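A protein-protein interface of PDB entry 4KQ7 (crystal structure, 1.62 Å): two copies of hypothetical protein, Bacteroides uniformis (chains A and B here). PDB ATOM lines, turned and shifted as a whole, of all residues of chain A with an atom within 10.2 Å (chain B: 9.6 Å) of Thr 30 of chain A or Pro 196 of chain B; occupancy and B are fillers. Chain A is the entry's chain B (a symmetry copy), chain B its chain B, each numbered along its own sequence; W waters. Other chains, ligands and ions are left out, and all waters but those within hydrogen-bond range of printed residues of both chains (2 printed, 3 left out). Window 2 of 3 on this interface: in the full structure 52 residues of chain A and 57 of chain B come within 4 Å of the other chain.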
ATOM      1  N   SER A  26      21.936  -0.468   4.291  1.00  0.00           N
ATOM      2  CA  SER A  26      23.044  -0.098   3.418  1.00  0.00           C
ATOM      3  C   SER A  26      23.943   0.943   4.128  1.00  0.00           C
ATOM      4  O   SER A  26      24.753   1.604   3.476  1.00  0.00           O
ATOM      5  CB  SER A  26      22.511   0.433   2.089  1.00  0.00           C
ATOM      6  OG  SER A  26      21.669   1.549   2.323  1.00  0.00           O
ATOM      7  N   THR A  27      23.821   1.059   5.465  1.00  0.00           N
ATOM      8  CA  THR A  27      24.631   1.983   6.285  1.00  0.00           C
ATOM      9  C   THR A  27      26.125   1.889   5.925  1.00  0.00           C
ATOM     10  O   THR A  27      26.652   0.781   5.760  1.00  0.00           O
ATOM     11  CB  THR A  27      24.445   1.708   7.820  1.00  0.00           C
ATOM     12  OG1 THR A  27      25.390   2.478   8.544  1.00  0.00           O
ATOM     13  CG2 THR A  27      24.724   0.278   8.216  1.00  0.00           C
ATOM     14  N   ASP A  28      26.813   3.037   5.852  1.00  0.00           N
ATOM     15  CA  ASP A  28      28.249   3.069   5.588  1.00  0.00           C
ATOM     16  C   ASP A  28      28.986   2.340   6.720  1.00  0.00           C
ATOM     17  O   ASP A  28      28.944   2.791   7.869  1.00  0.00           O
ATOM     18  CB  ASP A  28      28.733   4.517   5.457  1.00  0.00           C
ATOM     19  CG  ASP A  28      30.181   4.695   5.028  1.00  0.00           C
ATOM     20  OD1 ASP A  28      30.994   3.740   5.220  1.00  0.00           O
ATOM     21  OD2 ASP A  28      30.517   5.787   4.540  1.00  0.00           O
ATOM     22  N   PRO A  29      29.662   1.199   6.437  1.00  0.00           N
ATOM     23  CA  PRO A  29      30.326   0.457   7.539  1.00  0.00           C
ATOM     24  C   PRO A  29      31.460   1.234   8.218  1.00  0.00           C
ATOM     25  O   PRO A  29      31.839   0.898   9.343  1.00  0.00           O
ATOM     26  CB  PRO A  29      30.884  -0.799   6.854  1.00  0.00           C
ATOM     27  CG  PRO A  29      30.180  -0.885   5.537  1.00  0.00           C
ATOM     28  CD  PRO A  29      29.834   0.521   5.137  1.00  0.00           C
ATOM     29  N   THR A  30      32.017   2.250   7.536  1.00  0.00           N
ATOM     30  CA  THR A  30      33.125   3.044   8.117  1.00  0.00           C
ATOM     31  C   THR A  30      32.610   4.109   9.100  1.00  0.00           C
ATOM     32  O   THR A  30      33.399   4.692   9.861  1.00  0.00           O
ATOM     33  CB  THR A  30      33.939   3.743   7.009  1.00  0.00           C
ATOM     34  OG1 THR A  30      33.144   4.787   6.427  1.00  0.00           O
ATOM     35  CG2 THR A  30      34.434   2.784   5.921  1.00  0.00           C
ATOM     36  N   GLY A  31      31.313   4.385   9.051  1.00  0.00           N
ATOM     37  CA  GLY A  31      30.714   5.443   9.858  1.00  0.00           C
ATOM     38  C   GLY A  31      30.636   6.763   9.101  1.00  0.00           C
ATOM     39  O   GLY A  31      30.168   7.771   9.646  1.00  0.00           O
ATOM     40  N   GLY A  32      31.080   6.751   7.845  1.00  0.00           N
ATOM     41  CA  GLY A  32      30.993   7.910   6.957  1.00  0.00           C
ATOM     42  C   GLY A  32      29.572   8.069   6.439  1.00  0.00           C
ATOM     43  O   GLY A  32      28.650   7.423   6.953  1.00  0.00           O
ATOM     44  N   ASN A  33      29.390   8.899   5.407  1.00  0.00           N
ATOM     45  CA  ASN A  33      28.054   9.182   4.888  1.00  0.00           C
ATOM     46  C   ASN A  33      27.781   8.522   3.517  1.00  0.00           C
ATOM     47  O   ASN A  33      26.903   8.977   2.782  1.00  0.00           O
ATOM     48  CB  ASN A  33      27.824  10.702   4.810  1.00  0.00           C
ATOM     49  CG  ASN A  33      26.358  11.044   4.663  1.00  0.00           C
ATOM     50  OD1 ASN A  33      25.492  10.465   5.339  1.00  0.00           O
ATOM     51  ND2 ASN A  33      26.035  11.926   3.724  1.00  0.00           N
ATOM     52  N   ARG A  34      28.500   7.434   3.189  1.00  0.00           N
ATOM     53  CA  ARG A  34      28.232   6.718   1.926  1.00  0.00           C
ATOM     54  C   ARG A  34      27.269   5.574   2.293  1.00  0.00           C
ATOM     55  O   ARG A  34      27.650   4.400   2.322  1.00  0.00           O
ATOM     56  CB  ARG A  34      29.550   6.231   1.295  1.00  0.00           C
ATOM     57  CG  ARG A  34      29.383   5.660  -0.126  1.00  0.00           C
ATOM     58  CD  ARG A  34      30.735   5.263  -0.716  1.00  0.00           C
ATOM     59  NE  ARG A  34      30.583   4.522  -1.973  1.00  0.00           N
ATOM     60  CZ  ARG A  34      30.483   5.084  -3.177  1.00  0.00           C
ATOM     61  NH1 ARG A  34      30.533   6.407  -3.309  1.00  0.00           N
ATOM     62  NH2 ARG A  34      30.331   4.326  -4.260  1.00  0.00           N
ATOM     63  N   ASP A  35      26.038   5.942   2.674  1.00  0.00           N
ATOM     64  CA  ASP A  35      25.057   5.021   3.252  1.00  0.00           C
ATOM     65  C   ASP A  35      24.217   4.280   2.196  1.00  0.00           C
ATOM     66  O   ASP A  35      23.036   3.991   2.398  1.00  0.00           O
ATOM     67  CB  ASP A  35      24.170   5.768   4.252  1.00  0.00           C
ATOM     68  CG  ASP A  35      24.945   6.275   5.463  1.00  0.00           C
ATOM     69  OD1 ASP A  35      25.628   5.473   6.116  1.00  0.00           O
ATOM     70  OD2 ASP A  35      24.778   7.429   5.814  1.00  0.00           O
ATOM     71  N   HIS A  36      24.890   3.864   1.122  1.00  0.00           N
ATOM     72  CA  HIS A  36      24.275   3.096   0.042  1.00  0.00           C
ATOM     73  C   HIS A  36      25.249   2.037  -0.413  1.00  0.00           C
ATOM     74  O   HIS A  36      26.450   2.128  -0.140  1.00  0.00           O
ATOM     75  CB  HIS A  36      23.869   4.009  -1.128  1.00  0.00           C
ATOM     76  CG  HIS A  36      25.022   4.750  -1.734  1.00  0.00           C
ATOM     77  ND1 HIS A  36      25.842   4.159  -2.689  1.00  0.00           N
ATOM     78  CD2 HIS A  36      25.421   6.033  -1.545  1.00  0.00           C
ATOM     79  CE1 HIS A  36      26.725   5.093  -3.027  1.00  0.00           C
ATOM     80  NE2 HIS A  36      26.507   6.237  -2.373  1.00  0.00           N
ATOM     81  N   GLU A  38      27.483  -0.242  -3.149  1.00  0.00           N
ATOM     82  CA  GLU A  38      28.299   0.070  -4.315  1.00  0.00           C
ATOM     83  C   GLU A  38      27.463  -0.097  -5.598  1.00  0.00           C
ATOM     84  O   GLU A  38      26.458  -0.820  -5.578  1.00  0.00           O
ATOM     85  CB  GLU A  38      29.568  -0.808  -4.353  1.00  0.00           C
ATOM     86  CG  GLU A  38      30.612  -0.355  -3.346  1.00  0.00           C
ATOM     87  CD  GLU A  38      30.837   1.148  -3.278  1.00  0.00           C
ATOM     88  OE1 GLU A  38      31.255   1.737  -4.301  1.00  0.00           O
ATOM     89  OE2 GLU A  38      30.511   1.746  -2.226  1.00  0.00           O
ATOM     90  N   LEU B 181      30.310  20.933  13.889  1.00  0.00           N
ATOM     91  CA  LEU B 181      31.669  20.433  14.104  1.00  0.00           C
ATOM     92  C   LEU B 181      32.663  21.617  14.216  1.00  0.00           C
ATOM     93  O   LEU B 181      32.411  22.702  13.656  1.00  0.00           O
ATOM     94  CB  LEU B 181      32.088  19.518  12.928  1.00  0.00           C
ATOM     95  CG  LEU B 181      31.569  18.081  12.967  1.00  0.00           C
ATOM     96  CD1 LEU B 181      31.717  17.436  11.587  1.00  0.00           C
ATOM     97  CD2 LEU B 181      32.338  17.247  14.009  1.00  0.00           C
ATOM     98  N   GLU B 183      35.356  22.164  12.598  1.00  0.00           N
ATOM     99  CA  GLU B 183      35.741  22.533  11.222  1.00  0.00           C
ATOM    100  C   GLU B 183      34.559  23.156  10.435  1.00  0.00           C
ATOM    101  O   GLU B 183      34.722  23.458   9.244  1.00  0.00           O
ATOM    102  CB  GLU B 183      36.301  21.321  10.446  1.00  0.00           C
ATOM    103  CG  GLU B 183      35.340  20.140  10.311  1.00  0.00           C
ATOM    104  CD  GLU B 183      35.494  19.051  11.357  1.00  0.00           C
ATOM    105  OE1 GLU B 183      35.709  19.392  12.544  1.00  0.00           O
ATOM    106  OE2 GLU B 183      35.400  17.857  10.992  1.00  0.00           O
ATOM    107  N   THR B 186      30.268  20.860   7.427  1.00  0.00           N
ATOM    108  CA  THR B 186      30.848  20.195   6.258  1.00  0.00           C
ATOM    109  C   THR B 186      29.893  19.238   5.537  1.00  0.00           C
ATOM    110  O   THR B 186      30.369  18.334   4.840  1.00  0.00           O
ATOM    111  CB  THR B 186      32.111  19.444   6.674  1.00  0.00           C
ATOM    112  OG1 THR B 186      31.791  18.571   7.763  1.00  0.00           O
ATOM    113  CG2 THR B 186      33.249  20.398   7.060  1.00  0.00           C
ATOM    114  N   ALA B 193      36.376  18.631   4.144  1.00  0.00           N
ATOM    115  CA  ALA B 193      36.312  17.166   4.097  1.00  0.00           C
ATOM    116  C   ALA B 193      35.446  16.582   5.204  1.00  0.00           C
ATOM    117  O   ALA B 193      35.468  17.050   6.344  1.00  0.00           O
ATOM    118  CB  ALA B 193      37.713  16.561   4.158  1.00  0.00           C
ATOM    119  N   GLN B 194      34.665  15.565   4.838  1.00  0.00           N
ATOM    120  CA  GLN B 194      33.800  14.835   5.765  1.00  0.00           C
ATOM    121  C   GLN B 194      34.619  13.785   6.486  1.00  0.00           C
ATOM    122  O   GLN B 194      35.642  13.297   5.957  1.00  0.00           O
ATOM    123  CB  GLN B 194      32.625  14.188   5.025  1.00  0.00           C
ATOM    124  CG  GLN B 194      31.669  15.215   4.441  1.00  0.00           C
ATOM    125  CD  GLN B 194      30.492  14.544   3.804  1.00  0.00           C
ATOM    126  OE1 GLN B 194      30.551  14.139   2.655  1.00  0.00           O
ATOM    127  NE2 GLN B 194      29.396  14.424   4.545  1.00  0.00           N
ATOM    128  N   LYS B 195      34.179  13.455   7.707  1.00  0.00           N
ATOM    129  CA  LYS B 195      34.870  12.479   8.545  1.00  0.00           C
ATOM    130  C   LYS B 195      33.887  11.422   9.067  1.00  0.00           C
ATOM    131  O   LYS B 195      32.678  11.700   9.159  1.00  0.00           O
ATOM    132  CB  LYS B 195      35.590  13.181   9.715  1.00  0.00           C
ATOM    133  CG  LYS B 195      36.672  14.180   9.298  1.00  0.00           C
ATOM    134  CD  LYS B 195      38.034  13.516   9.071  1.00  0.00           C
ATOM    135  CE  LYS B 195      38.898  14.286   8.102  1.00  0.00           C
ATOM    136  NZ  LYS B 195      38.590  13.930   6.691  1.00  0.00           N
ATOM    137  N   PRO B 196      34.376  10.188   9.438  1.00  0.00           N
ATOM    138  CA  PRO B 196      33.428   9.179   9.937  1.00  0.00           C
ATOM    139  C   PRO B 196      32.964   9.434  11.369  1.00  0.00           C
ATOM    140  O   PRO B 196      33.705   9.977  12.201  1.00  0.00           O
ATOM    141  CB  PRO B 196      34.219   7.856   9.872  1.00  0.00           C
ATOM    142  CG  PRO B 196      35.660   8.258   9.979  1.00  0.00           C
ATOM    143  CD  PRO B 196      35.767   9.638   9.380  1.00  0.00           C
ATOM    144  N   ASN B 197      31.714   9.038  11.639  1.00  0.00           N
ATOM    145  CA  ASN B 197      31.114   9.051  12.972  1.00  0.00           C
ATOM    146  C   ASN B 197      31.259   7.634  13.490  1.00  0.00           C
ATOM    147  O   ASN B 197      30.470   6.766  13.120  1.00  0.00           O
ATOM    148  CB  ASN B 197      29.647   9.513  12.940  1.00  0.00           C
ATOM    149  CG  ASN B 197      28.962   9.503  14.291  1.00  0.00           C
ATOM    150  OD1 ASN B 197      29.581   9.268  15.331  1.00  0.00           O
ATOM    151  ND2 ASN B 197      27.664   9.787  14.302  1.00  0.00           N
ATOM    152  N   THR B 198      32.297   7.392  14.291  1.00  0.00           N
ATOM    153  CA  THR B 198      32.626   6.034  14.740  1.00  0.00           C
ATOM    154  C   THR B 198      32.055   5.669  16.124  1.00  0.00           C
ATOM    155  O   THR B 198      32.212   4.516  16.540  1.00  0.00           O
ATOM    156  CB  THR B 198      34.165   5.844  14.764  1.00  0.00           C
ATOM    157  OG1 THR B 198      34.735   6.802  15.661  1.00  0.00           O
ATOM    158  CG2 THR B 198      34.804   5.997  13.371  1.00  0.00           C
ATOM    159  N   THR B 199      31.418   6.622  16.835  1.00  0.00           N
ATOM    160  CA  THR B 199      30.902   6.363  18.189  1.00  0.00           C
ATOM    161  C   THR B 199      29.421   6.750  18.390  1.00  0.00           C
ATOM    162  O   THR B 199      28.770   6.220  19.298  1.00  0.00           O
ATOM    163  CB  THR B 199      31.731   7.134  19.226  1.00  0.00           C
ATOM    164  OG1 THR B 199      31.573   8.538  19.011  1.00  0.00           O
ATOM    165  CG2 THR B 199      33.226   6.744  19.235  1.00  0.00           C
ATOM    166  N   GLY B 200      28.936   7.718  17.602  1.00  0.00           N
ATOM    167  CA  GLY B 200      27.598   8.271  17.773  1.00  0.00           C
ATOM    168  C   GLY B 200      27.502   9.177  18.994  1.00  0.00           C
ATOM    169  O   GLY B 200      26.399   9.594  19.360  1.00  0.00           O
ATOM    170  N   GLU B 201      28.658   9.514  19.630  1.00  0.00           N
ATOM    171  CA  GLU B 201      28.670  10.296  20.875  1.00  0.00           C
ATOM    172  C   GLU B 201      28.084  11.698  20.733  1.00  0.00           C
ATOM    173  O   GLU B 201      27.547  12.218  21.722  1.00  0.00           O
ATOM    174  CB  GLU B 201      30.084  10.388  21.465  1.00  0.00           C
ATOM    175  CG  GLU B 201      30.494   9.137  22.222  1.00  0.00           C
ATOM    176  CD  GLU B 201      31.962   9.021  22.597  1.00  0.00           C
ATOM    177  OE1 GLU B 201      32.779   9.834  22.106  1.00  0.00           O
ATOM    178  OE2 GLU B 201      32.301   8.087  23.356  1.00  0.00           O
ATOM    179  N   ARG B 202      28.150  12.310  19.540  1.00  0.00           N
ATOM    180  CA  ARG B 202      27.611  13.649  19.366  1.00  0.00           C
ATOM    181  C   ARG B 202      26.188  13.629  18.770  1.00  0.00           C
ATOM    182  O   ARG B 202      25.635  14.694  18.462  1.00  0.00           O
ATOM    183  CB  ARG B 202      28.560  14.496  18.504  1.00  0.00           C
ATOM    184  CG  ARG B 202      29.889  14.817  19.230  1.00  0.00           C
ATOM    185  CD  ARG B 202      30.878  15.621  18.380  1.00  0.00           C
ATOM    186  NE  ARG B 202      30.339  16.926  17.985  1.00  0.00           N
ATOM    187  CZ  ARG B 202      29.865  17.206  16.775  1.00  0.00           C
ATOM    188  NH1 ARG B 202      29.894  16.288  15.814  1.00  0.00           N
ATOM    189  NH2 ARG B 202      29.373  18.409  16.510  1.00  0.00           N
ATOM    190  N   ASN B 203      25.590  12.429  18.609  1.00  0.00           N
ATOM    191  CA  ASN B 203      24.222  12.323  18.055  1.00  0.00           C
ATOM    192  C   ASN B 203      23.188  12.973  18.962  1.00  0.00           C
ATOM    193  O   ASN B 203      23.384  13.019  20.189  1.00  0.00           O
ATOM    194  CB  ASN B 203      23.811  10.852  17.908  1.00  0.00           C
ATOM    195  CG  ASN B 203      24.532  10.064  16.847  1.00  0.00           C
ATOM    196  OD1 ASN B 203      25.524  10.516  16.271  1.00  0.00           O
ATOM    197  ND2 ASN B 203      24.017   8.863  16.567  1.00  0.00           N
ATOM    198  N   ASP B 234      21.950   9.658  10.198  1.00  0.00           N
ATOM    199  CA  ASP B 234      21.422   8.314  10.417  1.00  0.00           C
ATOM    200  C   ASP B 234      20.801   8.165  11.779  1.00  0.00           C
ATOM    201  O   ASP B 234      21.370   8.675  12.758  1.00  0.00           O
ATOM    202  CB  ASP B 234      22.578   7.278  10.367  1.00  0.00           C
ATOM    203  CG  ASP B 234      23.444   7.277   9.125  1.00  0.00           C
ATOM    204  OD1 ASP B 234      22.991   7.801   8.084  1.00  0.00           O
ATOM    205  OD2 ASP B 234      24.542   6.695   9.179  1.00  0.00           O
ATOM    206  N   MET B 236      20.379   5.837  15.032  1.00  0.00           N
ATOM    207  CA  MET B 236      21.268   4.867  15.659  1.00  0.00           C
ATOM    208  C   MET B 236      20.673   4.462  17.006  1.00  0.00           C
ATOM    209  O   MET B 236      20.443   5.332  17.867  1.00  0.00           O
ATOM    210  CB  MET B 236      22.658   5.492  15.809  1.00  0.00           C
ATOM    211  CG  MET B 236      23.709   4.517  16.202  1.00  0.00           C
ATOM    212  SD  MET B 236      25.441   5.373  16.409  1.00  0.00           S
ATOM    213  CE  MET B 236      26.088   5.106  14.637  1.00  0.00           C
ATOM    214  N   ILE B 248      21.235   0.633  12.711  1.00  0.00           N
ATOM    215  CA  ILE B 248      21.862   1.836  12.147  1.00  0.00           C
ATOM    216  C   ILE B 248      21.210   2.132  10.814  1.00  0.00           C
ATOM    217  O   ILE B 248      21.135   1.262   9.953  1.00  0.00           O
ATOM    218  CB  ILE B 248      23.414   1.712  11.998  1.00  0.00           C
ATOM    219  CG1 ILE B 248      24.099   1.175  13.278  1.00  0.00           C
ATOM    220  CG2 ILE B 248      24.013   3.079  11.598  1.00  0.00           C
ATOM    221  CD1 ILE B 248      25.551   0.709  13.076  1.00  0.00           C
ATOM    222  N   GLU B 308      21.798  11.344  14.048  1.00  0.00           N
ATOM    223  CA  GLU B 308      22.777  12.373  13.707  1.00  0.00           C
ATOM    224  C   GLU B 308      22.083  13.677  13.320  1.00  0.00           C
ATOM    225  O   GLU B 308      21.014  13.638  12.698  1.00  0.00           O
ATOM    226  CB  GLU B 308      23.647  11.944  12.523  1.00  0.00           C
ATOM    227  CG  GLU B 308      24.634  10.826  12.793  1.00  0.00           C
ATOM    228  CD  GLU B 308      25.377  10.406  11.541  1.00  0.00           C
ATOM    229  OE1 GLU B 308      24.723  10.186  10.492  1.00  0.00           O
ATOM    230  OE2 GLU B 308      26.622  10.292  11.619  1.00  0.00           O
ATOM    231  N   GLY B 310      22.770  16.067  10.853  1.00  0.00           N
ATOM    232  CA  GLY B 310      23.610  16.180   9.670  1.00  0.00           C
ATOM    233  C   GLY B 310      24.597  15.022   9.695  1.00  0.00           C
ATOM    234  O   GLY B 310      24.816  14.427  10.761  1.00  0.00           O
ATOM    235  N   SER B 311      25.216  14.680   8.542  1.00  0.00           N
ATOM    236  CA  SER B 311      26.200  13.585   8.555  1.00  0.00           C
ATOM    237  C   SER B 311      27.342  13.906   9.529  1.00  0.00           C
ATOM    238  O   SER B 311      27.805  15.051   9.589  1.00  0.00           O
ATOM    239  CB  SER B 311      26.762  13.334   7.160  1.00  0.00           C
ATOM    240  OG  SER B 311      27.400  14.487   6.638  1.00  0.00           O
ATOM    241  N   ASN B 312      27.722  12.917  10.368  1.00  0.00           N
ATOM    242  CA  ASN B 312      28.751  13.081  11.413  1.00  0.00           C
ATOM    243  C   ASN B 312      28.439  14.318  12.304  1.00  0.00           C
ATOM    244  O   ASN B 312      29.354  15.002  12.771  1.00  0.00           O
ATOM    245  CB  ASN B 312      30.175  13.150  10.822  1.00  0.00           C
ATOM    246  CG  ASN B 312      31.251  13.125  11.894  1.00  0.00           C
ATOM    247  OD1 ASN B 312      31.074  12.528  12.966  1.00  0.00           O
ATOM    248  ND2 ASN B 312      32.340  13.852  11.676  1.00  0.00           N
ATOM    249  N   ASN B 313      27.130  14.620  12.495  1.00  0.00           N
ATOM    250  CA  ASN B 313      26.664  15.684  13.392  1.00  0.00           C
ATOM    251  C   ASN B 313      27.302  17.037  13.058  1.00  0.00           C
ATOM    252  O   ASN B 313      27.704  17.785  13.952  1.00  0.00           O
ATOM    253  CB  ASN B 313      26.991  15.262  14.845  1.00  0.00           C
ATOM    254  CG  ASN B 313      26.230  14.028  15.236  1.00  0.00           C
ATOM    255  OD1 ASN B 313      25.013  14.005  15.145  1.00  0.00           O
ATOM    256  ND2 ASN B 313      26.936  12.963  15.598  1.00  0.00           N
HETATM  257  O   HOH W   1      28.701  10.344   8.521  1.00  0.00           O
HETATM  258  O   HOH W   2      27.884  13.334   1.973  1.00  0.00           O
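O of Gly 31 of chain A sits at hydrogen-bond distance from N of Asn 197 of chain B (2.8 Å). The side-chain carboxylate of Asp 35 of chain A lies close to the side-chain carboxylate of Asp 234 of chain B, at 2.9 Å.
The backbone NH (N) of Asp 28 of chain A sits at hydrogen-bond distance from the side-chain carboxylate (OD1) of Asp 35 of chain A, at 2.7 Å. The side-chain carboxylate of Asp 28 of chain A lies within hydrogen-bond range of the side-chain hydroxyl of Thr 30 of chain A. NE2 of Gln 194 of chain B lies within hydrogen-bond range of OG of Ser 311 of chain B (2.9 Å). OG1 of Thr 30 of chain A lies within hydrogen-bond range of N of Gly 32 of chain A (3.2 Å). The backbone NH of Gly 32 of chain A lies close to the side-chain carboxylate of Asp 28 of chain A (3.5 Å). The side-chain hydroxyl (OG) of Ser 26 of chain A sits at hydrogen-bond distance from the backbone carbonyl oxygen (O) of Asp 35 of chain A (2.8 Å).
Among the printed residues, merely in contact across the chains: Thr 30 of chain A with Pro 196 of chain B (3.3 Å), Thr 27 of chain A with Ile 248 of chain B (3.4 Å), Asn 33 of chain A with Ser 311 of chain B (3.4 Å), Gly 31 of chain A with Pro 196 of chain B (3.6 Å), Gly 32 of chain A with Pro 196 of chain B (3.9 Å) and Thr 30 of chain A with Thr 198 of chain B (3.9996 Å).
Printed residues of chain B within 4 Å of Thr 27 of chain A: Ile 248. Asp 28 of chain A touches none of the printed residues of chain B. Of the printed residues of chain B, Thr 30 of chain A touches Pro 196 (3.3 Å) and Thr 198 (3.9996 Å). Of chain B, only Pro 196 (3.6 Å) and Asn 197 (2.8 Å) come within 4 Å of Gly 31 of chain A. Of the printed residues of chain B, Asn 33 of chain A touches Ser 311. Printed residues of chain B within 4 Å of Asp 35 of chain A: Asp 234 (2.9 Å). Pro 196 of chain B touches just these residues of chain A: Thr 30, Gly 31 and Gly 32. Asn 197 of chain B touches just one residue of chain A: Gly 31. The nearest printed residue of chain B that does not touch Thr 30 of chain A is Asn 197 of chain B (4.8 Å).
Among the printed residues, 8 pairs touch across the chains.
No position is printed for both chains.
Water W2 bridges OE1 of Gln 194 of chain B (2.9 Å) and ND2 of Asn 33 of chain A (2.9 Å). Water W1 lies within hydrogen-bond range of the backbone carbonyl oxygen (O) of Gly 31 of chain A, the backbone carbonyl oxygen (O) of Gly 32 of chain A and the backbone NH (N) of Asn 312 of chain B.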
